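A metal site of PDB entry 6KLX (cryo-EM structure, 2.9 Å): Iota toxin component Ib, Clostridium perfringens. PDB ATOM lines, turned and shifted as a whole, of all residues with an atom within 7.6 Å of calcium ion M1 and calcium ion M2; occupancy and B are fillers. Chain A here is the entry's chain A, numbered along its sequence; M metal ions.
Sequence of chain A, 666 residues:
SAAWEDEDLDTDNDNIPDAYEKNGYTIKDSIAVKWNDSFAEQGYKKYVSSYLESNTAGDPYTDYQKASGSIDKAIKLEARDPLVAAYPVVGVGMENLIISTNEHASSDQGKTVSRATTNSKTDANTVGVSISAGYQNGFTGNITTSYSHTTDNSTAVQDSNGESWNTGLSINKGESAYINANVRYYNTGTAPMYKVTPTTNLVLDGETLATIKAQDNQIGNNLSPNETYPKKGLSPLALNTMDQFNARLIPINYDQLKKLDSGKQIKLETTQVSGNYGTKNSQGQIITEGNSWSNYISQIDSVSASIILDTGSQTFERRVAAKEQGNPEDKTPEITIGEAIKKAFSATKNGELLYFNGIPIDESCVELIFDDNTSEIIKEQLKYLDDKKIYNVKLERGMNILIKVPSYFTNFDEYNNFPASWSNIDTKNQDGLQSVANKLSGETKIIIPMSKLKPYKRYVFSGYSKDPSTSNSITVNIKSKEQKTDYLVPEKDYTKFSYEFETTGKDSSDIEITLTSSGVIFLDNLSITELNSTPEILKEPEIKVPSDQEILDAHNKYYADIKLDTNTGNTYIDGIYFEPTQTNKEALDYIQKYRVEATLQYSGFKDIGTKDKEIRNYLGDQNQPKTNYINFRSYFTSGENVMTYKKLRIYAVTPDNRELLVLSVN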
ATOM      1  N   LEU A   9       2.952  30.455   1.550  1.00  0.00           N
ATOM      2  CA  LEU A   9       2.786  29.730   0.304  1.00  0.00           C
ATOM      3  C   LEU A   9       1.319  29.510  -0.003  1.00  0.00           C
ATOM      4  O   LEU A   9       0.526  29.155   0.873  1.00  0.00           O
ATOM      5  CB  LEU A   9       3.515  28.391   0.384  1.00  0.00           C
ATOM      6  CG  LEU A   9       3.529  27.536  -0.878  1.00  0.00           C
ATOM      7  CD1 LEU A   9       4.288  28.245  -1.976  1.00  0.00           C
ATOM      8  CD2 LEU A   9       4.147  26.192  -0.576  1.00  0.00           C
ATOM      9  N   ASP A  10       0.948  29.731  -1.265  1.00  0.00           N
ATOM     10  CA  ASP A  10      -0.412  29.528  -1.759  1.00  0.00           C
ATOM     11  C   ASP A  10      -0.303  28.704  -3.034  1.00  0.00           C
ATOM     12  O   ASP A  10      -0.010  29.236  -4.096  1.00  0.00           O
ATOM     13  CB  ASP A  10      -1.114  30.861  -2.007  1.00  0.00           C
ATOM     14  CG  ASP A  10      -2.582  30.699  -2.317  1.00  0.00           C
ATOM     15  OD1 ASP A  10      -3.151  29.649  -1.982  1.00  0.00           O
ATOM     16  OD2 ASP A  10      -3.169  31.634  -2.890  1.00  0.00           O
ATOM     17  N   THR A  11      -0.551  27.401  -2.921  1.00  0.00           N
ATOM     18  CA  THR A  11      -0.291  26.508  -4.048  1.00  0.00           C
ATOM     19  C   THR A  11      -1.377  26.615  -5.112  1.00  0.00           C
ATOM     20  O   THR A  11      -1.067  26.735  -6.307  1.00  0.00           O
ATOM     21  CB  THR A  11      -0.163  25.066  -3.548  1.00  0.00           C
ATOM     22  OG1 THR A  11       0.859  24.998  -2.549  1.00  0.00           O
ATOM     23  CG2 THR A  11       0.202  24.150  -4.682  1.00  0.00           C
ATOM     24  N   ASP A  12      -2.637  26.581  -4.721  1.00  0.00           N
ATOM     25  CA  ASP A  12      -3.741  26.581  -5.663  1.00  0.00           C
ATOM     26  C   ASP A  12      -4.178  27.978  -6.082  1.00  0.00           C
ATOM     27  O   ASP A  12      -5.106  28.109  -6.878  1.00  0.00           O
ATOM     28  CB  ASP A  12      -4.937  25.822  -5.082  1.00  0.00           C
ATOM     29  CG  ASP A  12      -5.258  26.252  -3.683  1.00  0.00           C
ATOM     30  OD1 ASP A  12      -4.415  26.937  -3.071  1.00  0.00           O
ATOM     31  OD2 ASP A  12      -6.349  25.915  -3.186  1.00  0.00           O
ATOM     32  N   ASN A  13      -3.523  29.022  -5.561  1.00  0.00           N
ATOM     33  CA  ASN A  13      -3.793  30.415  -5.925  1.00  0.00           C
ATOM     34  C   ASN A  13      -5.262  30.792  -5.699  1.00  0.00           C
ATOM     35  O   ASN A  13      -5.987  31.142  -6.626  1.00  0.00           O
ATOM     36  CB  ASN A  13      -3.387  30.679  -7.375  1.00  0.00           C
ATOM     37  CG  ASN A  13      -1.900  30.589  -7.599  1.00  0.00           C
ATOM     38  OD1 ASN A  13      -1.120  31.190  -6.867  1.00  0.00           O
ATOM     39  ND2 ASN A  13      -1.496  29.854  -8.621  1.00  0.00           N
ATOM     40  N   ASP A  14      -5.688  30.721  -4.435  1.00  0.00           N
ATOM     41  CA  ASP A  14      -7.042  31.132  -4.087  1.00  0.00           C
ATOM     42  C   ASP A  14      -7.054  31.991  -2.834  1.00  0.00           C
ATOM     43  O   ASP A  14      -8.048  32.027  -2.116  1.00  0.00           O
ATOM     44  CB  ASP A  14      -7.958  29.927  -3.942  1.00  0.00           C
ATOM     45  CG  ASP A  14      -7.603  29.067  -2.758  1.00  0.00           C
ATOM     46  OD1 ASP A  14      -6.425  29.001  -2.382  1.00  0.00           O
ATOM     47  OD2 ASP A  14      -8.516  28.442  -2.202  1.00  0.00           O
ATOM     48  N   ASN A  15      -5.951  32.668  -2.547  1.00  0.00           N
ATOM     49  CA  ASN A  15      -5.844  33.682  -1.496  1.00  0.00           C
ATOM     50  C   ASN A  15      -5.984  33.120  -0.089  1.00  0.00           C
ATOM     51  O   ASN A  15      -6.225  33.867   0.853  1.00  0.00           O
ATOM     52  CB  ASN A  15      -6.848  34.809  -1.705  1.00  0.00           C
ATOM     53  CG  ASN A  15      -6.697  35.488  -3.037  1.00  0.00           C
ATOM     54  OD1 ASN A  15      -5.583  35.755  -3.477  1.00  0.00           O
ATOM     55  ND2 ASN A  15      -7.811  35.766  -3.694  1.00  0.00           N
ATOM     56  N   ILE A  16      -5.824  31.814   0.087  1.00  0.00           N
ATOM     57  CA  ILE A  16      -5.722  31.206   1.399  1.00  0.00           C
ATOM     58  C   ILE A  16      -4.403  30.456   1.446  1.00  0.00           C
ATOM     59  O   ILE A  16      -4.157  29.599   0.597  1.00  0.00           O
ATOM     60  CB  ILE A  16      -6.891  30.265   1.720  1.00  0.00           C
ATOM     61  CG1 ILE A  16      -8.228  30.916   1.399  1.00  0.00           C
ATOM     62  CG2 ILE A  16      -6.857  29.888   3.181  1.00  0.00           C
ATOM     63  CD1 ILE A  16      -9.356  29.967   1.489  1.00  0.00           C
ATOM     64  N   PRO A  17      -3.526  30.734   2.412  1.00  0.00           N
ATOM     65  CA  PRO A  17      -2.242  30.021   2.475  1.00  0.00           C
ATOM     66  C   PRO A  17      -2.435  28.525   2.653  1.00  0.00           C
ATOM     67  O   PRO A  17      -3.492  28.051   3.067  1.00  0.00           O
ATOM     68  CB  PRO A  17      -1.569  30.639   3.705  1.00  0.00           C
ATOM     69  CG  PRO A  17      -2.159  31.975   3.815  1.00  0.00           C
ATOM     70  CD  PRO A  17      -3.579  31.831   3.382  1.00  0.00           C
ATOM     71  N   ASP A  18      -1.388  27.783   2.323  1.00  0.00           N
ATOM     72  CA  ASP A  18      -1.427  26.326   2.439  1.00  0.00           C
ATOM     73  C   ASP A  18      -1.570  25.892   3.887  1.00  0.00           C
ATOM     74  O   ASP A  18      -2.352  24.999   4.197  1.00  0.00           O
ATOM     75  CB  ASP A  18      -0.183  25.707   1.826  1.00  0.00           C
ATOM     76  CG  ASP A  18      -0.204  25.731   0.323  1.00  0.00           C
ATOM     77  OD1 ASP A  18      -1.103  26.383  -0.249  1.00  0.00           O
ATOM     78  OD2 ASP A  18       0.681  25.094  -0.296  1.00  0.00           O
ATOM     79  N   ALA A  19      -0.817  26.523   4.784  1.00  0.00           N
ATOM     80  CA  ALA A  19      -0.840  26.140   6.189  1.00  0.00           C
ATOM     81  C   ALA A  19      -2.150  26.486   6.879  1.00  0.00           C
ATOM     82  O   ALA A  19      -2.403  25.992   7.972  1.00  0.00           O
ATOM     83  CB  ALA A  19       0.309  26.809   6.934  1.00  0.00           C
ATOM     84  N   TYR A  20      -2.976  27.336   6.270  1.00  0.00           N
ATOM     85  CA  TYR A  20      -4.283  27.657   6.824  1.00  0.00           C
ATOM     86  C   TYR A  20      -5.342  26.664   6.397  1.00  0.00           C
ATOM     87  O   TYR A  20      -6.195  26.294   7.202  1.00  0.00           O
ATOM     88  CB  TYR A  20      -4.709  29.061   6.399  1.00  0.00           C
ATOM     89  CG  TYR A  20      -3.935  30.191   7.027  1.00  0.00           C
ATOM     90  CD1 TYR A  20      -2.849  29.958   7.833  1.00  0.00           C
ATOM     91  CD2 TYR A  20      -4.310  31.497   6.805  1.00  0.00           C
ATOM     92  CE1 TYR A  20      -2.140  30.996   8.405  1.00  0.00           C
ATOM     93  CE2 TYR A  20      -3.621  32.539   7.364  1.00  0.00           C
ATOM     94  CZ  TYR A  20      -2.532  32.287   8.154  1.00  0.00           C
ATOM     95  OH  TYR A  20      -1.844  33.329   8.712  1.00  0.00           O
ATOM     96  N   GLU A  21      -5.309  26.223   5.138  1.00  0.00           N
ATOM     97  CA  GLU A  21      -6.345  25.341   4.635  1.00  0.00           C
ATOM     98  C   GLU A  21      -6.268  23.959   5.263  1.00  0.00           C
ATOM     99  O   GLU A  21      -7.292  23.257   5.328  1.00  0.00           O
ATOM    100  CB  GLU A  21      -6.255  25.229   3.121  1.00  0.00           C
ATOM    101  CG  GLU A  21      -6.731  26.440   2.406  1.00  0.00           C
ATOM    102  CD  GLU A  21      -6.763  26.269   0.922  1.00  0.00           C
ATOM    103  OE1 GLU A  21      -7.732  25.678   0.412  1.00  0.00           O
ATOM    104  OE2 GLU A  21      -5.835  26.733   0.240  1.00  0.00           O
ATOM    105  N   TYR A  25      -8.874  27.928   9.510  1.00  0.00           N
ATOM    106  CA  TYR A  25      -8.825  29.367   9.293  1.00  0.00           C
ATOM    107  C   TYR A  25     -10.237  29.915   9.406  1.00  0.00           C
ATOM    108  O   TYR A  25     -11.211  29.167   9.488  1.00  0.00           O
ATOM    109  CB  TYR A  25      -8.224  29.715   7.934  1.00  0.00           C
ATOM    110  CG  TYR A  25      -9.022  29.203   6.756  1.00  0.00           C
ATOM    111  CD1 TYR A  25      -8.856  27.917   6.284  1.00  0.00           C
ATOM    112  CD2 TYR A  25      -9.933  30.014   6.115  1.00  0.00           C
ATOM    113  CE1 TYR A  25      -9.571  27.458   5.227  1.00  0.00           C
ATOM    114  CE2 TYR A  25     -10.657  29.550   5.055  1.00  0.00           C
ATOM    115  CZ  TYR A  25     -10.469  28.270   4.611  1.00  0.00           C
ATOM    116  OH  TYR A  25     -11.177  27.805   3.543  1.00  0.00           O
ATOM    117  N   SER A  49     -10.124  23.096   4.120  1.00  0.00           N
ATOM    118  CA  SER A  49     -10.337  22.774   2.719  1.00  0.00           C
ATOM    119  C   SER A  49      -9.026  22.250   2.153  1.00  0.00           C
ATOM    120  O   SER A  49      -8.004  22.206   2.836  1.00  0.00           O
ATOM    121  CB  SER A  49     -10.851  23.996   1.967  1.00  0.00           C
ATOM    122  OG  SER A  49      -9.917  25.050   2.023  1.00  0.00           O
ATOM    123  N   SER A  50      -9.070  21.825   0.893  1.00  0.00           N
ATOM    124  CA  SER A  50      -7.904  21.253   0.247  1.00  0.00           C
ATOM    125  C   SER A  50      -6.917  22.341  -0.138  1.00  0.00           C
ATOM    126  O   SER A  50      -7.277  23.294  -0.819  1.00  0.00           O
ATOM    127  CB  SER A  50      -8.322  20.460  -0.989  1.00  0.00           C
ATOM    128  OG  SER A  50      -7.202  19.940  -1.670  1.00  0.00           O
ATOM    129  N   TYR A  51      -5.670  22.186   0.287  1.00  0.00           N
ATOM    130  CA  TYR A  51      -4.674  23.188  -0.049  1.00  0.00           C
ATOM    131  C   TYR A  51      -4.083  22.992  -1.432  1.00  0.00           C
ATOM    132  O   TYR A  51      -3.217  23.777  -1.837  1.00  0.00           O
ATOM    133  CB  TYR A  51      -3.553  23.197   0.996  1.00  0.00           C
ATOM    134  CG  TYR A  51      -2.525  22.122   0.819  1.00  0.00           C
ATOM    135  CD1 TYR A  51      -2.722  20.844   1.306  1.00  0.00           C
ATOM    136  CD2 TYR A  51      -1.327  22.386   0.181  1.00  0.00           C
ATOM    137  CE1 TYR A  51      -1.783  19.867   1.154  1.00  0.00           C
ATOM    138  CE2 TYR A  51      -0.383  21.415   0.010  1.00  0.00           C
ATOM    139  CZ  TYR A  51      -0.612  20.155   0.496  1.00  0.00           C
ATOM    140  OH  TYR A  51       0.338  19.185   0.338  1.00  0.00           O
ATOM    141  N   LEU A  52      -4.537  21.989  -2.176  1.00  0.00           N
ATOM    142  CA  LEU A  52      -4.076  21.753  -3.535  1.00  0.00           C
ATOM    143  C   LEU A  52      -5.120  22.064  -4.586  1.00  0.00           C
ATOM    144  O   LEU A  52      -4.808  22.045  -5.774  1.00  0.00           O
ATOM    145  CB  LEU A  52      -3.621  20.300  -3.701  1.00  0.00           C
ATOM    146  CG  LEU A  52      -2.291  19.895  -3.095  1.00  0.00           C
ATOM    147  CD1 LEU A  52      -1.984  18.479  -3.473  1.00  0.00           C
ATOM    148  CD2 LEU A  52      -1.202  20.826  -3.565  1.00  0.00           C
ATOM    149  N   GLU A  53      -6.353  22.342  -4.181  1.00  0.00           N
ATOM    150  CA  GLU A  53      -7.454  22.570  -5.100  1.00  0.00           C
ATOM    151  C   GLU A  53      -8.176  23.857  -4.723  1.00  0.00           C
ATOM    152  O   GLU A  53      -8.446  24.098  -3.548  1.00  0.00           O
ATOM    153  CB  GLU A  53      -8.426  21.409  -5.080  1.00  0.00           C
ATOM    154  CG  GLU A  53      -9.472  21.495  -6.164  1.00  0.00           C
ATOM    155  CD  GLU A  53     -10.153  20.176  -6.395  1.00  0.00           C
ATOM    156  OE1 GLU A  53      -9.727  19.180  -5.779  1.00  0.00           O
ATOM    157  OE2 GLU A  53     -11.119  20.137  -7.192  1.00  0.00           O
ATOM    158  N   SER A  54      -8.481  24.669  -5.730  1.00  0.00           N
ATOM    159  CA  SER A  54      -9.163  25.934  -5.470  1.00  0.00           C
ATOM    160  C   SER A  54     -10.644  25.746  -5.231  1.00  0.00           C
ATOM    161  O   SER A  54     -11.255  26.527  -4.496  1.00  0.00           O
ATOM    162  CB  SER A  54      -8.935  26.892  -6.628  1.00  0.00           C
ATOM    163  OG  SER A  54      -9.642  26.478  -7.765  1.00  0.00           O
ATOM    164  N   ASN A  55     -11.252  24.733  -5.828  1.00  0.00           N
ATOM    165  CA  ASN A  55     -12.659  24.407  -5.620  1.00  0.00           C
ATOM    166  C   ASN A  55     -12.720  23.054  -4.936  1.00  0.00           C
ATOM    167  O   ASN A  55     -12.827  22.011  -5.599  1.00  0.00           O
ATOM    168  CB  ASN A  55     -13.417  24.398  -6.933  1.00  0.00           C
ATOM    169  CG  ASN A  55     -13.480  25.748  -7.591  1.00  0.00           C
ATOM    170  OD1 ASN A  55     -12.467  26.317  -7.972  1.00  0.00           O
ATOM    171  ND2 ASN A  55     -14.683  26.268  -7.733  1.00  0.00           N
ATOM    172  N   THR A  56     -12.659  23.057  -3.610  1.00  0.00           N
ATOM    173  CA  THR A  56     -12.628  21.808  -2.861  1.00  0.00           C
ATOM    174  C   THR A  56     -13.881  20.980  -3.090  1.00  0.00           C
ATOM    175  O   THR A  56     -13.798  19.753  -3.248  1.00  0.00           O
ATOM    176  CB  THR A  56     -12.475  22.113  -1.371  1.00  0.00           C
ATOM    177  OG1 THR A  56     -11.325  22.940  -1.175  1.00  0.00           O
ATOM    178  CG2 THR A  56     -12.299  20.840  -0.579  1.00  0.00           C
ATOM    179  N   THR A  62     -14.872  29.160  -5.448  1.00  0.00           N
ATOM    180  CA  THR A  62     -13.651  28.683  -4.835  1.00  0.00           C
ATOM    181  C   THR A  62     -13.837  28.570  -3.320  1.00  0.00           C
ATOM    182  O   THR A  62     -14.923  28.746  -2.779  1.00  0.00           O
ATOM    183  CB  THR A  62     -12.478  29.609  -5.181  1.00  0.00           C
ATOM    184  OG1 THR A  62     -12.581  30.822  -4.441  1.00  0.00           O
ATOM    185  CG2 THR A  62     -12.478  29.935  -6.642  1.00  0.00           C
ATOM    186  N   ASP A  63     -12.736  28.242  -2.628  1.00  0.00           N
ATOM    187  CA  ASP A  63     -12.784  28.181  -1.175  1.00  0.00           C
ATOM    188  C   ASP A  63     -12.919  29.569  -0.566  1.00  0.00           C
ATOM    189  O   ASP A  63     -13.688  29.766   0.382  1.00  0.00           O
ATOM    190  CB  ASP A  63     -11.542  27.491  -0.640  1.00  0.00           C
ATOM    191  CG  ASP A  63     -11.433  26.051  -1.079  1.00  0.00           C
ATOM    192  OD1 ASP A  63     -12.469  25.476  -1.457  1.00  0.00           O
ATOM    193  OD2 ASP A  63     -10.331  25.498  -1.033  1.00  0.00           O
ATOM    194  N   TYR A  64     -12.188  30.533  -1.110  1.00  0.00           N
ATOM    195  CA  TYR A  64     -12.213  31.876  -0.557  1.00  0.00           C
ATOM    196  C   TYR A  64     -13.539  32.568  -0.830  1.00  0.00           C
ATOM    197  O   TYR A  64     -14.000  33.364  -0.014  1.00  0.00           O
ATOM    198  CB  TYR A  64     -11.069  32.699  -1.138  1.00  0.00           C
ATOM    199  CG  TYR A  64     -11.048  34.104  -0.597  1.00  0.00           C
ATOM    200  CD1 TYR A  64     -10.514  34.378   0.650  1.00  0.00           C
ATOM    201  CD2 TYR A  64     -11.589  35.154  -1.316  1.00  0.00           C
ATOM    202  CE1 TYR A  64     -10.509  35.645   1.151  1.00  0.00           C
ATOM    203  CE2 TYR A  64     -11.583  36.421  -0.814  1.00  0.00           C
ATOM    204  CZ  TYR A  64     -11.043  36.668   0.415  1.00  0.00           C
ATOM    205  OH  TYR A  64     -11.028  37.939   0.919  1.00  0.00           O
ATOM    206  N   PRO A  82     -16.491  25.436   2.696  1.00  0.00           N
ATOM    207  CA  PRO A  82     -15.879  24.863   1.503  1.00  0.00           C
ATOM    208  C   PRO A  82     -16.181  23.385   1.288  1.00  0.00           C
ATOM    209  O   PRO A  82     -16.094  22.896   0.163  1.00  0.00           O
ATOM    210  CB  PRO A  82     -14.381  25.091   1.744  1.00  0.00           C
ATOM    211  CG  PRO A  82     -14.342  26.287   2.594  1.00  0.00           C
ATOM    212  CD  PRO A  82     -15.519  26.194   3.499  1.00  0.00           C
HETATM  213 CA    CA M   1      -8.120  25.426  -1.775  1.00  0.00          CA
HETATM  214 CA    CA M   2      -4.522  28.027  -1.115  1.00  0.00          CA
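Calcium ion M2 is bound by OD1 of Asp 12 (2.2 Å), OE2 of Glu 21 (2.3 Å), OD1 of Asp 10 (2.3 Å), O of Ile 16 (2.4 Å) and OD1 of Asp 14 (2.5 Å). Calcium ion M2 has five donor atoms within binding distance.
The backbone NH (N) of Ser 50 lies within hydrogen-bond range of the side-chain hydroxyl (OG1) of Thr 56, at 3.3 Å. The side-chain carboxylate (OD2) of Asp 63 lies close to the side-chain hydroxyl (OG) of Ser 49 (3.1 Å). The backbone NH of Asn 15 is in hydrogen-bond range of the side-chain carboxylate of Asp 10 (3.0 Å). OG of Ser 54 is in hydrogen-bond range of OD1 of Asn 55, 2.8 Å away. The backbone NH (N) of Asp 63 lies within hydrogen-bond range of the backbone carbonyl oxygen (O) of Ser 54 (2.9 Å). OD1 of Asp 18 is in hydrogen-bond range of N of Thr 11, 2.9 Å away. O of Glu 21 lies within hydrogen-bond range of N of Ser 49 (3.1 Å). The backbone carbonyl oxygen (O) of Leu 9 is in hydrogen-bond range of the backbone NH (N) of Asp 18 (2.8 Å).
Ser 54 touches calcium ion M1. Of the 26 residues printed, 7 come within 4 Å of calcium ion M1.
Asp 18 touches calcium ion M2. The nearest printed residue that does not touch calcium ion M2 is Pro 17 (4.3 Å).
The side-chain carboxylate (OE1) of Glu 21 is bound to calcium ion M1, 2.2 Å away. Calcium ion M1 is bound by the backbone carbonyl oxygen (O) of Glu 53 (2.2 Å). OD2 of Asp 12 is bound to calcium ion M1. Calcium ion M1 is bound by the side-chain carboxylate (OD2) of Asp 63, 2.3 Å away. The backbone carbonyl oxygen (O) of Ser 50 binds calcium ion M1, at 2.5 Å. Slightly farther from calcium ion M1 lies OD2 of Asp 14 (3.1 Å).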
